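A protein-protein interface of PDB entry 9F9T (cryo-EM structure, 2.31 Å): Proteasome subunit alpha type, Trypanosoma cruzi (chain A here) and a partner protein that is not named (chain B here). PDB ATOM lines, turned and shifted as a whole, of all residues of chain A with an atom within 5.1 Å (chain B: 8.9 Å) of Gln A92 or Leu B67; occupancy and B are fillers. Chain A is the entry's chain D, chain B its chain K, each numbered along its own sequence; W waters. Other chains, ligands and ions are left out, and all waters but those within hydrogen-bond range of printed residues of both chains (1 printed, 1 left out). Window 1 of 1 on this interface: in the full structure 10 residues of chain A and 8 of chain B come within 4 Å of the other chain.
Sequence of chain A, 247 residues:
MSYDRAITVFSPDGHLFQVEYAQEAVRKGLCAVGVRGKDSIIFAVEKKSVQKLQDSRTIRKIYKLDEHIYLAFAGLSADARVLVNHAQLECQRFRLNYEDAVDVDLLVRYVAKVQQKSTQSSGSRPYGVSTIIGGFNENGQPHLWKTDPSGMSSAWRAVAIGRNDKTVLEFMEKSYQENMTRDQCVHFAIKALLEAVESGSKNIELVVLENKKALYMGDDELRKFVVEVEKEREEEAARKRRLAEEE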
ATOM      1  N   ASP A  66      26.233   0.088  12.006  1.00  0.00           N
ATOM      2  CA  ASP A  66      25.848   1.427  12.409  1.00  0.00           C
ATOM      3  C   ASP A  66      24.724   1.833  11.460  1.00  0.00           C
ATOM      4  O   ASP A  66      24.343   1.024  10.633  1.00  0.00           O
ATOM      5  CB  ASP A  66      27.033   2.406  12.432  1.00  0.00           C
ATOM      6  CG  ASP A  66      26.804   3.675  13.265  1.00  0.00           C
ATOM      7  OD1 ASP A  66      25.636   3.940  13.662  1.00  0.00           O
ATOM      8  OD2 ASP A  66      27.802   4.408  13.542  1.00  0.00           O
ATOM      9  N   GLN A  88      31.084  -2.937  15.827  1.00  0.00           N
ATOM     10  CA  GLN A  88      30.060  -2.124  16.477  1.00  0.00           C
ATOM     11  C   GLN A  88      30.684  -1.254  17.583  1.00  0.00           C
ATOM     12  O   GLN A  88      30.413  -0.047  17.658  1.00  0.00           O
ATOM     13  CB  GLN A  88      29.004  -3.105  16.983  1.00  0.00           C
ATOM     14  CG  GLN A  88      28.042  -3.564  15.892  1.00  0.00           C
ATOM     15  CD  GLN A  88      27.134  -4.706  16.295  1.00  0.00           C
ATOM     16  OE1 GLN A  88      27.352  -5.366  17.309  1.00  0.00           O
ATOM     17  NE2 GLN A  88      26.091  -4.925  15.500  1.00  0.00           N
ATOM     18  N   LEU A  89      31.483  -1.850  18.480  1.00  0.00           N
ATOM     19  CA  LEU A  89      32.255  -1.027  19.386  1.00  0.00           C
ATOM     20  C   LEU A  89      33.014   0.081  18.665  1.00  0.00           C
ATOM     21  O   LEU A  89      32.891   1.250  19.022  1.00  0.00           O
ATOM     22  CB  LEU A  89      33.242  -1.827  20.202  1.00  0.00           C
ATOM     23  CG  LEU A  89      32.689  -2.533  21.433  1.00  0.00           C
ATOM     24  CD1 LEU A  89      33.818  -3.272  22.173  1.00  0.00           C
ATOM     25  CD2 LEU A  89      32.013  -1.547  22.358  1.00  0.00           C
ATOM     26  N   GLU A  90      33.784  -0.256  17.650  1.00  0.00           N
ATOM     27  CA  GLU A  90      34.606   0.731  16.964  1.00  0.00           C
ATOM     28  C   GLU A  90      33.775   1.878  16.461  1.00  0.00           C
ATOM     29  O   GLU A  90      34.244   2.995  16.597  1.00  0.00           O
ATOM     30  CB  GLU A  90      35.318   0.185  15.733  1.00  0.00           C
ATOM     31  CG  GLU A  90      36.077   1.226  14.968  1.00  0.00           C
ATOM     32  CD  GLU A  90      37.108   2.040  15.766  1.00  0.00           C
ATOM     33  OE1 GLU A  90      36.944   3.315  15.864  1.00  0.00           O
ATOM     34  OE2 GLU A  90      38.072   1.418  16.281  1.00  0.00           O
ATOM     35  N   CYS A  91      32.612   1.648  15.841  1.00  0.00           N
ATOM     36  CA  CYS A  91      31.850   2.770  15.315  1.00  0.00           C
ATOM     37  C   CYS A  91      31.394   3.723  16.414  1.00  0.00           C
ATOM     38  O   CYS A  91      31.255   4.921  16.198  1.00  0.00           O
ATOM     39  CB  CYS A  91      30.538   2.364  14.662  1.00  0.00           C
ATOM     40  SG  CYS A  91      30.807   1.428  13.152  1.00  0.00           S
ATOM     41  N   GLN A  92      31.052   3.173  17.572  1.00  0.00           N
ATOM     42  CA  GLN A  92      30.514   3.993  18.635  1.00  0.00           C
ATOM     43  C   GLN A  92      31.680   4.718  19.292  1.00  0.00           C
ATOM     44  O   GLN A  92      31.565   5.907  19.559  1.00  0.00           O
ATOM     45  CB  GLN A  92      29.672   3.129  19.596  1.00  0.00           C
ATOM     46  CG  GLN A  92      28.357   2.658  18.975  1.00  0.00           C
ATOM     47  CD  GLN A  92      27.579   3.844  18.477  1.00  0.00           C
ATOM     48  OE1 GLN A  92      27.738   4.935  19.016  1.00  0.00           O
ATOM     49  NE2 GLN A  92      26.714   3.651  17.484  1.00  0.00           N
ATOM     50  N   ARG A  93      32.792   4.023  19.536  1.00  0.00           N
ATOM     51  CA  ARG A  93      34.014   4.701  19.963  1.00  0.00           C
ATOM     52  C   ARG A  93      34.314   5.944  19.101  1.00  0.00           C
ATOM     53  O   ARG A  93      34.676   7.015  19.601  1.00  0.00           O
ATOM     54  CB  ARG A  93      35.217   3.778  19.839  1.00  0.00           C
ATOM     55  CG  ARG A  93      36.183   3.903  20.997  1.00  0.00           C
ATOM     56  CD  ARG A  93      37.283   2.850  20.906  1.00  0.00           C
ATOM     57  NE  ARG A  93      36.813   1.457  20.936  1.00  0.00           N
ATOM     58  CZ  ARG A  93      37.227   0.490  20.109  1.00  0.00           C
ATOM     59  NH1 ARG A  93      38.071   0.748  19.120  1.00  0.00           N
ATOM     60  NH2 ARG A  93      36.791  -0.748  20.265  1.00  0.00           N
ATOM     61  N   PHE A  94      34.163   5.808  17.794  1.00  0.00           N
ATOM     62  CA  PHE A  94      34.496   6.891  16.912  1.00  0.00           C
ATOM     63  C   PHE A  94      33.510   8.057  17.120  1.00  0.00           C
ATOM     64  O   PHE A  94      33.895   9.230  17.229  1.00  0.00           O
ATOM     65  CB  PHE A  94      34.548   6.314  15.504  1.00  0.00           C
ATOM     66  CG  PHE A  94      35.021   7.240  14.423  1.00  0.00           C
ATOM     67  CD1 PHE A  94      36.290   7.133  13.898  1.00  0.00           C
ATOM     68  CD2 PHE A  94      34.163   8.141  13.839  1.00  0.00           C
ATOM     69  CE1 PHE A  94      36.689   7.948  12.853  1.00  0.00           C
ATOM     70  CE2 PHE A  94      34.572   8.968  12.788  1.00  0.00           C
ATOM     71  CZ  PHE A  94      35.836   8.872  12.306  1.00  0.00           C
ATOM     72  N   ARG A  95      32.213   7.783  17.223  1.00  0.00           N
ATOM     73  CA  ARG A  95      31.293   8.885  17.476  1.00  0.00           C
ATOM     74  C   ARG A  95      31.705   9.668  18.727  1.00  0.00           C
ATOM     75  O   ARG A  95      31.708  10.869  18.745  1.00  0.00           O
ATOM     76  CB  ARG A  95      29.857   8.377  17.586  1.00  0.00           C
ATOM     77  CG  ARG A  95      29.013   8.704  16.372  1.00  0.00           C
ATOM     78  CD  ARG A  95      27.584   8.501  16.799  1.00  0.00           C
ATOM     79  NE  ARG A  95      26.888   7.751  15.768  1.00  0.00           N
ATOM     80  CZ  ARG A  95      26.359   8.289  14.686  1.00  0.00           C
ATOM     81  NH1 ARG A  95      26.071   7.525  13.650  1.00  0.00           N
ATOM     82  NH2 ARG A  95      26.205   9.598  14.614  1.00  0.00           N
ATOM     83  N   LEU A  96      32.088   8.956  19.758  1.00  0.00           N
ATOM     84  CA  LEU A  96      32.486   9.512  21.038  1.00  0.00           C
ATOM     85  C   LEU A  96      33.785  10.307  20.944  1.00  0.00           C
ATOM     86  O   LEU A  96      33.888  11.368  21.522  1.00  0.00           O
ATOM     87  CB  LEU A  96      32.599   8.310  21.988  1.00  0.00           C
ATOM     88  CG  LEU A  96      32.209   8.561  23.436  1.00  0.00           C
ATOM     89  CD1 LEU A  96      30.858   9.249  23.504  1.00  0.00           C
ATOM     90  CD2 LEU A  96      32.221   7.274  24.244  1.00  0.00           C
ATOM     91  N   GLU B  59      26.727  12.066  25.895  1.00  0.00           N
ATOM     92  CA  GLU B  59      27.283  11.343  24.755  1.00  0.00           C
ATOM     93  C   GLU B  59      27.556   9.888  25.109  1.00  0.00           C
ATOM     94  O   GLU B  59      27.255   9.002  24.328  1.00  0.00           O
ATOM     95  CB  GLU B  59      28.548  12.028  24.219  1.00  0.00           C
ATOM     96  CG  GLU B  59      28.279  13.108  23.168  1.00  0.00           C
ATOM     97  CD  GLU B  59      29.475  13.269  22.208  1.00  0.00           C
ATOM     98  OE1 GLU B  59      29.366  12.950  20.949  1.00  0.00           O
ATOM     99  OE2 GLU B  59      30.568  13.658  22.713  1.00  0.00           O
ATOM    100  N   TYR B  60      28.109   9.649  26.278  1.00  0.00           N
ATOM    101  CA  TYR B  60      28.203   8.322  26.828  1.00  0.00           C
ATOM    102  C   TYR B  60      26.857   7.605  26.987  1.00  0.00           C
ATOM    103  O   TYR B  60      26.735   6.465  26.605  1.00  0.00           O
ATOM    104  CB  TYR B  60      28.879   8.541  28.160  1.00  0.00           C
ATOM    105  CG  TYR B  60      28.964   7.279  28.968  1.00  0.00           C
ATOM    106  CD1 TYR B  60      29.851   6.280  28.607  1.00  0.00           C
ATOM    107  CD2 TYR B  60      28.149   7.084  30.087  1.00  0.00           C
ATOM    108  CE1 TYR B  60      29.932   5.097  29.338  1.00  0.00           C
ATOM    109  CE2 TYR B  60      28.210   5.908  30.818  1.00  0.00           C
ATOM    110  CZ  TYR B  60      29.102   4.905  30.432  1.00  0.00           C
ATOM    111  OH  TYR B  60      29.191   3.725  31.120  1.00  0.00           O
ATOM    112  N   ILE B  61      25.819   8.205  27.500  1.00  0.00           N
ATOM    113  CA  ILE B  61      24.520   7.571  27.430  1.00  0.00           C
ATOM    114  C   ILE B  61      24.145   7.262  25.988  1.00  0.00           C
ATOM    115  O   ILE B  61      23.598   6.229  25.737  1.00  0.00           O
ATOM    116  CB  ILE B  61      23.410   8.439  28.111  1.00  0.00           C
ATOM    117  CG1 ILE B  61      23.776   8.804  29.541  1.00  0.00           C
ATOM    118  CG2 ILE B  61      22.053   7.753  28.162  1.00  0.00           C
ATOM    119  CD1 ILE B  61      24.136   7.561  30.361  1.00  0.00           C
ATOM    120  N   LYS B  62      24.237   8.215  25.069  1.00  0.00           N
ATOM    121  CA  LYS B  62      23.719   7.964  23.733  1.00  0.00           C
ATOM    122  C   LYS B  62      24.405   6.773  23.072  1.00  0.00           C
ATOM    123  O   LYS B  62      23.757   5.970  22.428  1.00  0.00           O
ATOM    124  CB  LYS B  62      23.939   9.111  22.768  1.00  0.00           C
ATOM    125  CG  LYS B  62      23.031  10.302  23.014  1.00  0.00           C
ATOM    126  CD  LYS B  62      23.316  11.601  22.217  1.00  0.00           C
ATOM    127  CE  LYS B  62      22.857  11.537  20.773  1.00  0.00           C
ATOM    128  NZ  LYS B  62      21.701  10.606  20.576  1.00  0.00           N
ATOM    129  N   CYS B  63      25.710   6.674  23.212  1.00  0.00           N
ATOM    130  CA  CYS B  63      26.452   5.679  22.488  1.00  0.00           C
ATOM    131  C   CYS B  63      26.152   4.312  23.073  1.00  0.00           C
ATOM    132  O   CYS B  63      25.863   3.428  22.300  1.00  0.00           O
ATOM    133  CB  CYS B  63      27.929   6.105  22.383  1.00  0.00           C
ATOM    134  SG  CYS B  63      28.081   7.649  21.384  1.00  0.00           S
ATOM    135  N   ASN B  64      26.159   4.130  24.398  1.00  0.00           N
ATOM    136  CA  ASN B  64      25.760   2.874  25.012  1.00  0.00           C
ATOM    137  C   ASN B  64      24.319   2.460  24.707  1.00  0.00           C
ATOM    138  O   ASN B  64      24.047   1.277  24.663  1.00  0.00           O
ATOM    139  CB  ASN B  64      25.954   2.888  26.514  1.00  0.00           C
ATOM    140  CG  ASN B  64      27.438   2.860  26.839  1.00  0.00           C
ATOM    141  OD1 ASN B  64      28.015   1.796  27.071  1.00  0.00           O
ATOM    142  ND2 ASN B  64      28.093   4.013  26.787  1.00  0.00           N
ATOM    143  N   MET B  65      23.392   3.379  24.501  1.00  0.00           N
ATOM    144  CA  MET B  65      22.061   2.964  24.141  1.00  0.00           C
ATOM    145  C   MET B  65      22.046   2.518  22.691  1.00  0.00           C
ATOM    146  O   MET B  65      21.263   1.674  22.317  1.00  0.00           O
ATOM    147  CB  MET B  65      21.040   4.111  24.273  1.00  0.00           C
ATOM    148  CG  MET B  65      20.678   4.367  25.735  1.00  0.00           C
ATOM    149  SD  MET B  65      19.550   5.724  25.894  1.00  0.00           S
ATOM    150  CE  MET B  65      18.104   4.904  25.204  1.00  0.00           C
ATOM    151  N   ALA B  66      22.812   3.206  21.860  1.00  0.00           N
ATOM    152  CA  ALA B  66      22.867   2.898  20.457  1.00  0.00           C
ATOM    153  C   ALA B  66      23.466   1.508  20.259  1.00  0.00           C
ATOM    154  O   ALA B  66      22.985   0.708  19.457  1.00  0.00           O
ATOM    155  CB  ALA B  66      23.639   3.967  19.734  1.00  0.00           C
ATOM    156  N   LEU B  67      24.414   1.174  21.105  1.00  0.00           N
ATOM    157  CA  LEU B  67      25.075  -0.105  21.043  1.00  0.00           C
ATOM    158  C   LEU B  67      24.134  -1.169  21.556  1.00  0.00           C
ATOM    159  O   LEU B  67      24.258  -2.304  21.174  1.00  0.00           O
ATOM    160  CB  LEU B  67      26.364   0.006  21.847  1.00  0.00           C
ATOM    161  CG  LEU B  67      27.346  -1.142  21.653  1.00  0.00           C
ATOM    162  CD1 LEU B  67      27.978  -1.050  20.281  1.00  0.00           C
ATOM    163  CD2 LEU B  67      28.410  -1.137  22.736  1.00  0.00           C
ATOM    164  N   LYS B  68      23.195  -0.837  22.439  1.00  0.00           N
ATOM    165  CA  LYS B  68      22.243  -1.820  22.945  1.00  0.00           C
ATOM    166  C   LYS B  68      21.155  -2.073  21.903  1.00  0.00           C
ATOM    167  O   LYS B  68      20.446  -3.060  21.962  1.00  0.00           O
ATOM    168  CB  LYS B  68      21.569  -1.354  24.230  1.00  0.00           C
ATOM    169  CG  LYS B  68      21.358  -2.440  25.268  1.00  0.00           C
ATOM    170  CD  LYS B  68      20.319  -2.088  26.353  1.00  0.00           C
ATOM    171  CE  LYS B  68      19.555  -3.301  26.860  1.00  0.00           C
ATOM    172  NZ  LYS B  68      18.240  -2.919  27.441  1.00  0.00           N
ATOM    173  N   ARG B  69      20.993  -1.195  20.948  1.00  0.00           N
ATOM    174  CA  ARG B  69      19.883  -1.333  20.036  1.00  0.00           C
ATOM    175  C   ARG B  69      20.299  -2.167  18.832  1.00  0.00           C
ATOM    176  O   ARG B  69      19.423  -2.692  18.161  1.00  0.00           O
ATOM    177  CB  ARG B  69      19.488   0.002  19.396  1.00  0.00           C
ATOM    178  CG  ARG B  69      18.504   0.852  20.159  1.00  0.00           C
ATOM    179  CD  ARG B  69      17.793   1.771  19.165  1.00  0.00           C
ATOM    180  NE  ARG B  69      18.675   2.545  18.304  1.00  0.00           N
ATOM    181  CZ  ARG B  69      19.347   3.641  18.669  1.00  0.00           C
ATOM    182  NH1 ARG B  69      20.084   4.286  17.777  1.00  0.00           N
ATOM    183  NH2 ARG B  69      19.277   4.095  19.914  1.00  0.00           N
ATOM    184  N   MET B  70      21.582  -2.151  18.434  1.00  0.00           N
ATOM    185  CA  MET B  70      22.008  -3.067  17.380  1.00  0.00           C
ATOM    186  C   MET B  70      22.272  -4.454  17.936  1.00  0.00           C
ATOM    187  O   MET B  70      21.987  -5.425  17.252  1.00  0.00           O
ATOM    188  CB  MET B  70      23.242  -2.684  16.572  1.00  0.00           C
ATOM    189  CG  MET B  70      24.265  -1.900  17.274  1.00  0.00           C
ATOM    190  SD  MET B  70      25.072  -0.950  15.999  1.00  0.00           S
ATOM    191  CE  MET B  70      23.690  -0.109  15.225  1.00  0.00           C
ATOM    192  N   ARG B  71      22.761  -4.560  19.150  1.00  0.00           N
ATOM    193  CA  ARG B  71      22.854  -5.864  19.763  1.00  0.00           C
ATOM    194  C   ARG B  71      21.468  -6.284  20.252  1.00  0.00           C
ATOM    195  O   ARG B  71      21.314  -6.773  21.382  1.00  0.00           O
ATOM    196  CB  ARG B  71      23.921  -5.799  20.854  1.00  0.00           C
ATOM    197  CG  ARG B  71      25.220  -5.193  20.338  1.00  0.00           C
ATOM    198  CD  ARG B  71      26.463  -5.992  20.675  1.00  0.00           C
ATOM    199  NE  ARG B  71      27.054  -5.587  21.938  1.00  0.00           N
ATOM    200  CZ  ARG B  71      28.277  -5.086  22.056  1.00  0.00           C
ATOM    201  NH1 ARG B  71      28.763  -4.807  23.254  1.00  0.00           N
ATOM    202  NH2 ARG B  71      29.005  -4.881  20.967  1.00  0.00           N
ATOM    203  N   GLU B  72      20.448  -6.095  19.397  1.00  0.00           N
ATOM    204  CA  GLU B  72      19.063  -6.362  19.793  1.00  0.00           C
ATOM    205  C   GLU B  72      18.066  -5.928  18.703  1.00  0.00           C
ATOM    206  O   GLU B  72      16.898  -5.672  18.985  1.00  0.00           O
ATOM    207  CB  GLU B  72      18.771  -5.691  21.148  1.00  0.00           C
ATOM    208  CG  GLU B  72      17.802  -6.485  22.023  1.00  0.00           C
ATOM    209  CD  GLU B  72      17.825  -6.226  23.523  1.00  0.00           C
ATOM    210  OE1 GLU B  72      16.995  -6.862  24.232  1.00  0.00           O
ATOM    211  OE2 GLU B  72      18.673  -5.421  23.991  1.00  0.00           O
ATOM    212  N   HIS B  73      18.548  -5.833  17.452  1.00  0.00           N
ATOM    213  CA  HIS B  73      17.731  -5.671  16.255  1.00  0.00           C
ATOM    214  C   HIS B  73      16.858  -4.415  16.323  1.00  0.00           C
ATOM    215  O   HIS B  73      15.751  -4.395  15.779  1.00  0.00           O
ATOM    216  CB  HIS B  73      17.007  -6.994  15.969  1.00  0.00           C
ATOM    217  CG  HIS B  73      17.968  -8.117  16.191  1.00  0.00           C
ATOM    218  ND1 HIS B  73      19.200  -8.143  15.564  1.00  0.00           N
ATOM    219  CD2 HIS B  73      17.951  -9.164  17.029  1.00  0.00           C
ATOM    220  CE1 HIS B  73      19.885  -9.196  15.981  1.00  0.00           C
ATOM    221  NE2 HIS B  73      19.142  -9.832  16.868  1.00  0.00           N
ATOM    222  N   GLY B  74      17.371  -3.364  16.965  1.00  0.00           N
ATOM    223  CA  GLY B  74      16.733  -2.055  16.923  1.00  0.00           C
ATOM    224  C   GLY B  74      15.543  -1.947  17.874  1.00  0.00           C
ATOM    225  O   GLY B  74      14.723  -1.040  17.748  1.00  0.00           O
ATOM    226  N   ARG B  75      15.486  -2.859  18.847  1.00  0.00           N
ATOM    227  CA  ARG B  75      14.396  -2.848  19.796  1.00  0.00           C
ATOM    228  C   ARG B  75      14.605  -1.686  20.761  1.00  0.00           C
ATOM    229  O   ARG B  75      15.675  -1.553  21.340  1.00  0.00           O
ATOM    230  CB  ARG B  75      14.281  -4.212  20.485  1.00  0.00           C
ATOM    231  CG  ARG B  75      12.905  -4.849  20.312  1.00  0.00           C
ATOM    232  CD  ARG B  75      12.440  -4.904  18.857  1.00  0.00           C
ATOM    233  NE  ARG B  75      11.208  -5.663  18.647  1.00  0.00           N
ATOM    234  CZ  ARG B  75      11.062  -6.661  17.779  1.00  0.00           C
ATOM    235  NH1 ARG B  75      12.079  -7.054  17.030  1.00  0.00           N
ATOM    236  NH2 ARG B  75       9.892  -7.266  17.666  1.00  0.00           N
ATOM    237  N   ILE B  77      14.460   0.506  23.998  1.00  0.00           N
ATOM    238  CA  ILE B  77      14.581   0.260  25.409  1.00  0.00           C
ATOM    239  C   ILE B  77      13.558   1.087  26.168  1.00  0.00           C
ATOM    240  O   ILE B  77      13.189   2.192  25.770  1.00  0.00           O
ATOM    241  CB  ILE B  77      16.033   0.543  25.778  1.00  0.00           C
ATOM    242  CG1 ILE B  77      16.236   0.888  27.245  1.00  0.00           C
ATOM    243  CG2 ILE B  77      16.616   1.582  24.854  1.00  0.00           C
ATOM    244  CD1 ILE B  77      17.709   1.086  27.622  1.00  0.00           C
ATOM    245  N   PHE B  85      20.023   2.783  33.842  1.00  0.00           N
ATOM    246  CA  PHE B  85      21.364   2.851  33.278  1.00  0.00           C
ATOM    247  C   PHE B  85      22.034   4.178  33.618  1.00  0.00           C
ATOM    248  O   PHE B  85      23.197   4.221  33.943  1.00  0.00           O
ATOM    249  CB  PHE B  85      21.271   2.586  31.774  1.00  0.00           C
ATOM    250  CG  PHE B  85      22.630   2.614  31.111  1.00  0.00           C
ATOM    251  CD1 PHE B  85      23.504   1.554  31.244  1.00  0.00           C
ATOM    252  CD2 PHE B  85      23.114   3.762  30.528  1.00  0.00           C
ATOM    253  CE1 PHE B  85      24.786   1.593  30.710  1.00  0.00           C
ATOM    254  CE2 PHE B  85      24.404   3.805  30.003  1.00  0.00           C
ATOM    255  CZ  PHE B  85      25.241   2.725  30.093  1.00  0.00           C
HETATM  256  O   HOH W   1      27.811   0.313  16.421  1.00  0.00           O
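Water W1 lies within hydrogen-bond range of the backbone carbonyl oxygen of Gln A88 (2.9 Å) and the side-chain sulfur of Met B70 (3.0 Å).
Of the 19 printed residues of chain B, 7 touch a printed residue of chain A.
Printed residues of chain B that touch a printed residue of chain A: Glu B59, Tyr B60, Cys B63, Ala B66, Leu B67, Met B70 and Arg B71.
Hydrophobic or aromatic side chains of chain B that line the printed part of chain A: Ala B66, Leu B67 and Met B70.
Printed residues of chain A that touch a printed residue of chain B: Asp A66, Gln A88, Leu A89, Gln A92, Arg A95 and Leu A96.
Hydrophobic or aromatic side chains of chain A within 4 Å of the printed part of chain B: Leu A89 and Leu A96.
Along chain A the printed residues that touch a printed residue of chain B span positions 66 to 96.
Among the printed residues, no Asp or Glu carboxylate lies within 4 Å of a Lys or Arg side-chain nitrogen of the other chain.
Of the printed residues of chain B, Gln A88 touches Leu B67, Met B70 and Arg B71.
No residue of chain B comes within 4 Å of Cys A91.
Of chain B, only Cys B63 (3.6 Å), Ala B66 (3.8 Å) and Leu B67 (3.9 Å) come within 4 Å of Gln A92.
Arg A93 touches none of the printed residues of chain B.
Of the printed residues of chain B, Leu A96 touches Glu B59 (3.7 Å), Tyr B60 (3.9 Å) and Cys B63 (3.8 Å).
Of the printed residues of chain A, Cys B63 touches Gln A92 and Leu A96.
Printed residues of chain A within 4 Å of Ala B66: Gln A92 (3.8 Å).
Leu B67 touches just these residues of chain A: Gln A88 (3.7 Å), Leu A89 (3.6 Å) and Gln A92 (3.9 Å).
Of the printed residues of chain A, Arg B71 touches Gln A88.
The nearest printed residue of chain A that does not touch Leu B67 is Glu A90 (6.4 Å).
The nearest printed residue of chain B that does not touch Leu A96 is Asn B64 (5.8 Å).
OE1 of Gln A92 lies close to SG of Cys B63, 3.6 Å away.
Among the printed residues, merely in contact across the chains: Asp A66 with Met B70, Gln A88 with Leu B67, Gln A88 with Met B70, Gln A88 with Arg B71, Leu A89 with Leu B67, Gln A92 with Ala B66, Gln A92 with Leu B67, Arg A95 with Glu B59, Leu A96 with Glu B59, Leu A96 with Tyr B60 and Leu A96 with Cys B63.
The side-chain sulfur (SG) of Cys B63 lies within hydrogen-bond range of the backbone carbonyl oxygen (O) of Glu B59 (3.3 Å).
The backbone carbonyl oxygen (O) of Tyr B60 lies within hydrogen-bond range of the side-chain amide nitrogen (ND2) of Asn B64.
The side-chain carboxylate (OD2) of Asp A66 is in salt-bridge range of the guanidinium group (NH1) of Arg A95 (3.6 Å).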
